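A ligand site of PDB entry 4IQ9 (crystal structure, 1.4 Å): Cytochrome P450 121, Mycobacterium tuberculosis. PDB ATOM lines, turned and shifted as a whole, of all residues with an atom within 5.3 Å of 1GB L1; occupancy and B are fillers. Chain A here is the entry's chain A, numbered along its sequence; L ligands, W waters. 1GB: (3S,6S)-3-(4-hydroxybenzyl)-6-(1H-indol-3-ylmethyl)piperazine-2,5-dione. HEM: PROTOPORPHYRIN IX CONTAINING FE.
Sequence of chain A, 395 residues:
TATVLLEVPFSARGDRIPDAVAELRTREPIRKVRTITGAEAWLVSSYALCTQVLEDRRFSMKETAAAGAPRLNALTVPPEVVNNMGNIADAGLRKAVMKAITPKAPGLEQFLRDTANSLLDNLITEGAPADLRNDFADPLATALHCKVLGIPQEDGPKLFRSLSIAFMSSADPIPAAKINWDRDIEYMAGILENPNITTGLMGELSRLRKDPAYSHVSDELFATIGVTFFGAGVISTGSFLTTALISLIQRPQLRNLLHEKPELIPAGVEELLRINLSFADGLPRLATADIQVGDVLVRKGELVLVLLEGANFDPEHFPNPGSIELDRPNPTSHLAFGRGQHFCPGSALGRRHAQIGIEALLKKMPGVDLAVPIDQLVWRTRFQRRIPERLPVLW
The backbone carbonyl oxygen (O) of Val 82 is in hydrogen-bond range of a nitrogen (NE1) of 1GB L1, at 3.2 Å.
SD of Met 61 sits close to NE1 of 1GB L1, at 3.7 Å.
NH1 of Arg 385 lies within hydrogen-bond range of OA of 1GB L1 (3.4 Å).
N of Gln 384 lies within hydrogen-bond range of O of Phe 167, at 2.7 Å.
The backbone carbonyl oxygen of Ala 232 lies within hydrogen-bond range of the side-chain hydroxyl of Ser 236, at 2.7 Å.
The guanidinium group (NH1) of Arg 385 is in hydrogen-bond range of the side-chain hydroxyl (OG) of Ser 236 (2.9 Å).
O of Ala 166 lies within hydrogen-bond range of OG1 of Thr 76, 2.8 Å away.
OG1 of Thr 228 sits at hydrogen-bond distance from ND2 of Asn 84 (2.9 Å).
Thr 76 touches 1GB L1.
Val 77 touches 1GB L1 (CG1 to CZB, 3.6 Å).
Val 81 touches 1GB L1 (O to CZ2, 3.6 Å).
Asn 84 touches 1GB L1 (ND2 to CH2, 3.3 Å).
Ala 166 touches 1GB L1 (O to CE3, 3.4 Å).
Phe 167 touches 1GB L1.
Thr 228 touches 1GB L1 (CB to CH2, 3.8 Å).
Ala 232 touches 1GB L1.
Gln 384 touches 1GB L1 (NE2 to CAB, 3.3 Å).
The nearest printed residue that does not touch 1GB L1 is Trp 181 (4.2 Å).
Water W7 bridges an oxygen (OB) of 1GB L1 (2.7 Å) and the side-chain amide oxygen of Gln 384 (3.2 Å).
Water W3 lies within hydrogen-bond range of OA of 1GB L1 (2.7 Å) and NH1 of Arg 385 (3.3 Å).
Water W10 bridges O2A of HEM L2 (2.6 Å) and NA of 1GB L1 (2.8 Å).
Water W2 lies within hydrogen-bond range of the backbone carbonyl oxygen of Thr 76 (2.8 Å) and an oxygen (OHB) of 1GB L1 (3.1 Å).
Water W9 lies within hydrogen-bond range of OG of Ser 236 (2.8 Å) and OA of 1GB L1 (3.4 Å).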
ATOM      1  N   MET A  61       7.004  -7.654 -24.305  1.00  0.00           N
ATOM      2  CA  MET A  61       7.907  -8.576 -23.618  1.00  0.00           C
ATOM      3  C   MET A  61       8.961  -9.043 -24.648  1.00  0.00           C
ATOM      4  O   MET A  61      10.155  -9.065 -24.359  1.00  0.00           O
ATOM      5  CB  MET A  61       7.145  -9.797 -23.046  1.00  0.00           C
ATOM      6  CG  MET A  61       8.086 -11.023 -22.681  1.00  0.00           C
ATOM      7  SD  MET A  61       7.188 -12.532 -22.215  1.00  0.00           S
ATOM      8  CE  MET A  61       6.511 -12.000 -20.703  1.00  0.00           C
ATOM      9  N   THR A  76      19.242 -15.642 -19.751  1.00  0.00           N
ATOM     10  CA  THR A  76      19.768 -16.963 -19.369  1.00  0.00           C
ATOM     11  C   THR A  76      19.226 -18.022 -20.343  1.00  0.00           C
ATOM     12  O   THR A  76      19.457 -19.220 -20.160  1.00  0.00           O
ATOM     13  CB  THR A  76      19.406 -17.336 -17.921  1.00  0.00           C
ATOM     14  OG1 THR A  76      17.995 -17.485 -17.822  1.00  0.00           O
ATOM     15  CG2 THR A  76      19.915 -16.307 -16.921  1.00  0.00           C
ATOM     16  N   VAL A  77      18.522 -17.574 -21.406  1.00  0.00           N
ATOM     17  CA  VAL A  77      17.967 -18.420 -22.448  1.00  0.00           C
ATOM     18  C   VAL A  77      18.307 -17.784 -23.779  1.00  0.00           C
ATOM     19  O   VAL A  77      18.555 -16.573 -23.835  1.00  0.00           O
ATOM     20  CB  VAL A  77      16.420 -18.576 -22.304  1.00  0.00           C
ATOM     21  CG1 VAL A  77      16.051 -19.324 -21.017  1.00  0.00           C
ATOM     22  CG2 VAL A  77      15.673 -17.228 -22.379  1.00  0.00           C
ATOM     23  N   VAL A  81      13.578 -17.429 -27.076  1.00  0.00           N
ATOM     24  CA  VAL A  81      12.862 -18.125 -26.006  1.00  0.00           C
ATOM     25  C   VAL A  81      12.149 -17.120 -25.079  1.00  0.00           C
ATOM     26  O   VAL A  81      11.182 -17.481 -24.414  1.00  0.00           O
ATOM     27  CB  VAL A  81      13.792 -19.128 -25.276  1.00  0.00           C
ATOM     28  CG1 VAL A  81      13.103 -19.809 -24.092  1.00  0.00           C
ATOM     29  CG2 VAL A  81      14.306 -20.178 -26.244  1.00  0.00           C
ATOM     30  N   VAL A  82      12.542 -15.822 -25.121  1.00  0.00           N
ATOM     31  CA  VAL A  82      11.851 -14.816 -24.324  1.00  0.00           C
ATOM     32  C   VAL A  82      10.373 -14.779 -24.811  1.00  0.00           C
ATOM     33  O   VAL A  82       9.444 -14.715 -23.990  1.00  0.00           O
ATOM     34  CB  VAL A  82      12.569 -13.453 -24.459  1.00  0.00           C
ATOM     35  CG1 VAL A  82      11.727 -12.315 -23.874  1.00  0.00           C
ATOM     36  CG2 VAL A  82      13.924 -13.506 -23.756  1.00  0.00           C
ATOM     37  N   ASN A  84       8.615 -17.276 -25.845  1.00  0.00           N
ATOM     38  CA  ASN A  84       8.178 -18.662 -25.824  1.00  0.00           C
ATOM     39  C   ASN A  84       6.681 -18.875 -26.036  1.00  0.00           C
ATOM     40  O   ASN A  84       6.279 -19.679 -26.889  1.00  0.00           O
ATOM     41  CB  ASN A  84       8.643 -19.281 -24.506  1.00  0.00           C
ATOM     42  CG  ASN A  84       8.515 -20.772 -24.425  1.00  0.00           C
ATOM     43  OD1 ASN A  84       8.876 -21.510 -25.345  1.00  0.00           O
ATOM     44  ND2 ASN A  84       8.070 -21.244 -23.252  1.00  0.00           N
ATOM     45  N   MET A  85       5.838 -18.160 -25.275  1.00  0.00           N
ATOM     46  CA  MET A  85       4.396 -18.337 -25.431  1.00  0.00           C
ATOM     47  C   MET A  85       3.882 -17.922 -26.783  1.00  0.00           C
ATOM     48  O   MET A  85       3.021 -18.608 -27.346  1.00  0.00           O
ATOM     49  CB  MET A  85       3.628 -17.648 -24.328  1.00  0.00           C
ATOM     50  CG  MET A  85       3.487 -18.519 -23.116  1.00  0.00           C
ATOM     51  SD  MET A  85       2.542 -20.083 -23.211  1.00  0.00           S
ATOM     52  CE  MET A  85       1.414 -19.805 -24.607  1.00  0.00           C
ATOM     53  N   ALA A 166      19.525 -21.103 -13.655  1.00  0.00           N
ATOM     54  CA  ALA A 166      18.676 -20.691 -14.776  1.00  0.00           C
ATOM     55  C   ALA A 166      17.845 -19.468 -14.444  1.00  0.00           C
ATOM     56  O   ALA A 166      17.560 -18.657 -15.334  1.00  0.00           O
ATOM     57  CB  ALA A 166      17.771 -21.845 -15.169  1.00  0.00           C
ATOM     58  N   PHE A 167      17.406 -19.358 -13.169  1.00  0.00           N
ATOM     59  CA  PHE A 167      16.570 -18.247 -12.758  1.00  0.00           C
ATOM     60  C   PHE A 167      17.333 -17.163 -12.016  1.00  0.00           C
ATOM     61  O   PHE A 167      16.716 -16.323 -11.344  1.00  0.00           O
ATOM     62  CB  PHE A 167      15.303 -18.739 -12.016  1.00  0.00           C
ATOM     63  CG  PHE A 167      14.375 -19.424 -12.984  1.00  0.00           C
ATOM     64  CD1 PHE A 167      14.480 -20.788 -13.214  1.00  0.00           C
ATOM     65  CD2 PHE A 167      13.486 -18.691 -13.741  1.00  0.00           C
ATOM     66  CE1 PHE A 167      13.658 -21.418 -14.173  1.00  0.00           C
ATOM     67  CE2 PHE A 167      12.646 -19.334 -14.671  1.00  0.00           C
ATOM     68  CZ  PHE A 167      12.786 -20.679 -14.898  1.00  0.00           C
ATOM     69  N   TRP A 181      21.307 -25.400 -19.993  1.00  0.00           N
ATOM     70  CA  TRP A 181      20.234 -25.252 -20.998  1.00  0.00           C
ATOM     71  C   TRP A 181      20.422 -26.280 -22.106  1.00  0.00           C
ATOM     72  O   TRP A 181      19.492 -27.021 -22.456  1.00  0.00           O
ATOM     73  CB  TRP A 181      20.228 -23.834 -21.574  1.00  0.00           C
ATOM     74  CG  TRP A 181      19.235 -23.646 -22.694  1.00  0.00           C
ATOM     75  CD1 TRP A 181      19.492 -23.722 -24.031  1.00  0.00           C
ATOM     76  CD2 TRP A 181      17.834 -23.385 -22.551  1.00  0.00           C
ATOM     77  NE1 TRP A 181      18.323 -23.503 -24.741  1.00  0.00           N
ATOM     78  CE2 TRP A 181      17.287 -23.332 -23.852  1.00  0.00           C
ATOM     79  CE3 TRP A 181      16.988 -23.201 -21.453  1.00  0.00           C
ATOM     80  CZ2 TRP A 181      15.918 -23.090 -24.082  1.00  0.00           C
ATOM     81  CZ3 TRP A 181      15.627 -22.978 -21.676  1.00  0.00           C
ATOM     82  CH2 TRP A 181      15.108 -22.932 -22.986  1.00  0.00           C
ATOM     83  N   THR A 228      11.215 -25.148 -20.620  1.00  0.00           N
ATOM     84  CA  THR A 228      10.649 -23.908 -20.066  1.00  0.00           C
ATOM     85  C   THR A 228       9.471 -24.144 -19.134  1.00  0.00           C
ATOM     86  O   THR A 228       9.358 -23.441 -18.128  1.00  0.00           O
ATOM     87  CB  THR A 228      10.292 -22.923 -21.162  1.00  0.00           C
ATOM     88  OG1 THR A 228       9.310 -23.522 -22.021  1.00  0.00           O
ATOM     89  CG2 THR A 228      11.517 -22.471 -21.959  1.00  0.00           C
ATOM     90  N   ALA A 232       9.940 -22.914 -15.367  1.00  0.00           N
ATOM     91  CA  ALA A 232       9.075 -21.824 -14.889  1.00  0.00           C
ATOM     92  C   ALA A 232       8.054 -22.358 -13.872  1.00  0.00           C
ATOM     93  O   ALA A 232       7.852 -21.729 -12.827  1.00  0.00           O
ATOM     94  CB  ALA A 232       8.340 -21.167 -16.052  1.00  0.00           C
ATOM     95  N   SER A 236       8.376 -21.337  -9.891  1.00  0.00           N
ATOM     96  CA  SER A 236       7.305 -20.454  -9.451  1.00  0.00           C
ATOM     97  C   SER A 236       6.458 -21.074  -8.357  1.00  0.00           C
ATOM     98  O   SER A 236       6.149 -20.384  -7.359  1.00  0.00           O
ATOM     99  CB  SER A 236       6.431 -20.029 -10.623  1.00  0.00           C
ATOM    100  OG  SER A 236       7.198 -19.357 -11.623  1.00  0.00           O
ATOM    101  N   PHE A 279       8.229 -12.600  -6.675  1.00  0.00           N
ATOM    102  CA  PHE A 279       8.950 -12.030  -7.829  1.00  0.00           C
ATOM    103  C   PHE A 279       9.919 -10.977  -7.325  1.00  0.00           C
ATOM    104  O   PHE A 279       9.517  -9.995  -6.722  1.00  0.00           O
ATOM    105  CB  PHE A 279       7.976 -11.475  -8.889  1.00  0.00           C
ATOM    106  CG  PHE A 279       7.524 -12.507  -9.898  1.00  0.00           C
ATOM    107  CD1 PHE A 279       6.748 -13.583  -9.503  1.00  0.00           C
ATOM    108  CD2 PHE A 279       7.909 -12.415 -11.224  1.00  0.00           C
ATOM    109  CE1 PHE A 279       6.365 -14.563 -10.434  1.00  0.00           C
ATOM    110  CE2 PHE A 279       7.490 -13.368 -12.162  1.00  0.00           C
ATOM    111  CZ  PHE A 279       6.744 -14.442 -11.746  1.00  0.00           C
ATOM    112  N   GLN A 384      15.647 -14.374  -9.736  1.00  0.00           N
ATOM    113  CA  GLN A 384      14.360 -13.894 -10.261  1.00  0.00           C
ATOM    114  C   GLN A 384      13.227 -14.102  -9.244  1.00  0.00           C
ATOM    115  O   GLN A 384      12.125 -13.575  -9.446  1.00  0.00           O
ATOM    116  CB  GLN A 384      14.031 -14.562 -11.590  1.00  0.00           C
ATOM    117  CG  GLN A 384      14.944 -14.086 -12.707  1.00  0.00           C
ATOM    118  CD  GLN A 384      14.776 -14.830 -14.018  1.00  0.00           C
ATOM    119  OE1 GLN A 384      15.780 -15.149 -14.702  1.00  0.00           O
ATOM    120  NE2 GLN A 384      13.540 -15.106 -14.389  1.00  0.00           N
ATOM    121  N   ARG A 385      13.498 -14.868  -8.189  1.00  0.00           N
ATOM    122  CA  ARG A 385      12.559 -15.047  -7.112  1.00  0.00           C
ATOM    123  C   ARG A 385      13.216 -14.706  -5.787  1.00  0.00           C
ATOM    124  O   ARG A 385      14.443 -14.788  -5.644  1.00  0.00           O
ATOM    125  CB  ARG A 385      12.027 -16.502  -7.010  1.00  0.00           C
ATOM    126  CG  ARG A 385      11.267 -16.984  -8.263  1.00  0.00           C
ATOM    127  CD  ARG A 385       9.920 -16.248  -8.441  1.00  0.00           C
ATOM    128  NE  ARG A 385       9.211 -16.755  -9.614  1.00  0.00           N
ATOM    129  CZ  ARG A 385       9.437 -16.368 -10.864  1.00  0.00           C
ATOM    130  NH1 ARG A 385       8.782 -16.940 -11.881  1.00  0.00           N
ATOM    131  NH2 ARG A 385      10.345 -15.416 -11.126  1.00  0.00           N
HETATM  132  OB  1GB L   1      12.018 -13.676 -17.981  1.00  0.00           O
HETATM  133  CB  1GB L   1      11.318 -14.557 -17.413  1.00  0.00           C
HETATM  134  CAB 1GB L   1      11.762 -15.927 -17.099  1.00  0.00           C
HETATM  135  CBB 1GB L   1      12.111 -16.655 -18.462  1.00  0.00           C
HETATM  136  CGB 1GB L   1      12.885 -17.916 -18.307  1.00  0.00           C
HETATM  137  CD4 1GB L   1      12.409 -19.167 -18.645  1.00  0.00           C
HETATM  138  CE4 1GB L   1      13.125 -20.331 -18.523  1.00  0.00           C
HETATM  139  CZB 1GB L   1      14.496 -20.217 -17.953  1.00  0.00           C
HETATM  140  OHB 1GB L   1      15.232 -21.314 -17.822  1.00  0.00           O
HETATM  141  CE3 1GB L   1      15.050 -18.997 -17.565  1.00  0.00           C
HETATM  142  CD3 1GB L   1      14.208 -17.835 -17.772  1.00  0.00           C
HETATM  143  NB  1GB L   1      10.813 -16.704 -16.367  1.00  0.00           N
HETATM  144  CA  1GB L   1       9.600 -16.483 -15.941  1.00  0.00           C
HETATM  145  OA  1GB L   1       8.995 -17.367 -15.289  1.00  0.00           O
HETATM  146  NA  1GB L   1       9.996 -14.188 -17.005  1.00  0.00           N
HETATM  147  CAA 1GB L   1       9.028 -15.074 -16.315  1.00  0.00           C
HETATM  148  CBA 1GB L   1       7.779 -15.275 -17.373  1.00  0.00           C
HETATM  149  CGA 1GB L   1       8.253 -15.720 -18.752  1.00  0.00           C
HETATM  150  CD2 1GB L   1       8.504 -16.996 -19.240  1.00  0.00           C
HETATM  151  CE2 1GB L   1       8.402 -18.310 -18.687  1.00  0.00           C
HETATM  152  CZ3 1GB L   1       8.733 -19.470 -19.492  1.00  0.00           C
HETATM  153  CH2 1GB L   1       9.167 -19.294 -20.848  1.00  0.00           C
HETATM  154  CZ2 1GB L   1       9.254 -17.957 -21.359  1.00  0.00           C
HETATM  155  CE1 1GB L   1       8.938 -16.843 -20.588  1.00  0.00           C
HETATM  156  NE1 1GB L   1       8.953 -15.547 -20.934  1.00  0.00           N
HETATM  157  CD1 1GB L   1       8.527 -14.826 -19.816  1.00  0.00           C
HETATM  158  CHA HEM L   2       4.133 -16.116 -16.807  1.00  0.00           C
HETATM  159  CHB HEM L   2       3.527 -15.996 -11.985  1.00  0.00           C
HETATM  160  CHC HEM L   2       3.139 -20.852 -12.025  1.00  0.00           C
HETATM  161  CHD HEM L   2       4.420 -20.925 -16.698  1.00  0.00           C
HETATM  162  C1A HEM L   2       3.902 -15.649 -15.508  1.00  0.00           C
HETATM  163  C2A HEM L   2       3.779 -14.275 -15.116  1.00  0.00           C
HETATM  164  C3A HEM L   2       3.678 -14.243 -13.768  1.00  0.00           C
HETATM  165  C4A HEM L   2       3.661 -15.594 -13.317  1.00  0.00           C
HETATM  166  CMA HEM L   2       3.558 -13.025 -12.869  1.00  0.00           C
HETATM  167  CAA HEM L   2       3.753 -13.085 -16.058  1.00  0.00           C
HETATM  168  CBA HEM L   2       5.151 -12.650 -16.530  1.00  0.00           C
HETATM  169  CGA HEM L   2       5.080 -11.390 -17.366  1.00  0.00           C
HETATM  170  O1A HEM L   2       4.005 -10.943 -17.787  1.00  0.00           O
HETATM  171  O2A HEM L   2       6.271 -10.833 -17.621  1.00  0.00           O
HETATM  172  C1B HEM L   2       3.461 -17.359 -11.567  1.00  0.00           C
HETATM  173  C2B HEM L   2       3.178 -17.740 -10.208  1.00  0.00           C
HETATM  174  C3B HEM L   2       3.024 -19.100 -10.215  1.00  0.00           C
HETATM  175  C4B HEM L   2       3.266 -19.507 -11.618  1.00  0.00           C
HETATM  176  CMB HEM L   2       3.061 -16.794  -9.036  1.00  0.00           C
HETATM  177  CAB HEM L   2       2.714 -20.038  -9.126  1.00  0.00           C
HETATM  178  CBB HEM L   2       2.359 -19.753  -7.911  1.00  0.00           C
HETATM  179  C1C HEM L   2       3.392 -21.298 -13.311  1.00  0.00           C
HETATM  180  C2C HEM L   2       3.306 -22.678 -13.720  1.00  0.00           C
HETATM  181  C3C HEM L   2       3.746 -22.692 -15.055  1.00  0.00           C
HETATM  182  C4C HEM L   2       4.003 -21.333 -15.447  1.00  0.00           C
HETATM  183  CMC HEM L   2       2.864 -23.844 -12.881  1.00  0.00           C
HETATM  184  CAC HEM L   2       3.862 -23.852 -15.988  1.00  0.00           C
HETATM  185  CBC HEM L   2       3.785 -25.156 -15.654  1.00  0.00           C
HETATM  186  C1D HEM L   2       4.566 -19.615 -17.079  1.00  0.00           C
HETATM  187  C2D HEM L   2       4.929 -19.192 -18.431  1.00  0.00           C
HETATM  188  C3D HEM L   2       4.723 -17.845 -18.498  1.00  0.00           C
HETATM  189  C4D HEM L   2       4.343 -17.450 -17.131  1.00  0.00           C
HETATM  190  CMD HEM L   2       5.353 -20.152 -19.544  1.00  0.00           C
HETATM  191  CAD HEM L   2       4.947 -16.919 -19.701  1.00  0.00           C
HETATM  192  CBD HEM L   2       3.595 -16.553 -20.341  1.00  0.00           C
HETATM  193  CGD HEM L   2       3.604 -15.581 -21.557  1.00  0.00           C
HETATM  194  O1D HEM L   2       2.548 -15.426 -22.149  1.00  0.00           O
HETATM  195  O2D HEM L   2       4.738 -15.040 -21.845  1.00  0.00           O
HETATM  196  NA  HEM L   2       3.800 -16.470 -14.380  1.00  0.00           N
HETATM  197  NB  HEM L   2       3.533 -18.448 -12.413  1.00  0.00           N
HETATM  198  NC  HEM L   2       3.760 -20.480 -14.359  1.00  0.00           N
HETATM  199  ND  HEM L   2       4.259 -18.518 -16.310  1.00  0.00           N
HETATM  200 FE   HEM L   2       3.709 -18.476 -14.392  1.00  0.00          FE
HETATM  201  O   HOH W   1      10.183 -11.972 -14.935  1.00  0.00           O
HETATM  202  O   HOH W   2      18.235 -21.007 -18.335  1.00  0.00           O
HETATM  203  O   HOH W   3       6.871 -15.968 -14.377  1.00  0.00           O
HETATM  204  O   HOH W   4       6.669 -16.018 -23.423  1.00  0.00           O
HETATM  205  O   HOH W   5      13.764 -23.859 -17.353  1.00  0.00           O
HETATM  206  O   HOH W   6      10.924 -14.374 -13.724  1.00  0.00           O
HETATM  207  O   HOH W   7      14.605 -13.867 -17.373  1.00  0.00           O
HETATM  208  O   HOH W   8      14.243 -14.262 -19.941  1.00  0.00           O
HETATM  209  O   HOH W   9       6.006 -18.457 -14.043  1.00  0.00           O
HETATM  210  O   HOH W  10       8.708 -11.734 -17.182  1.00  0.00           O
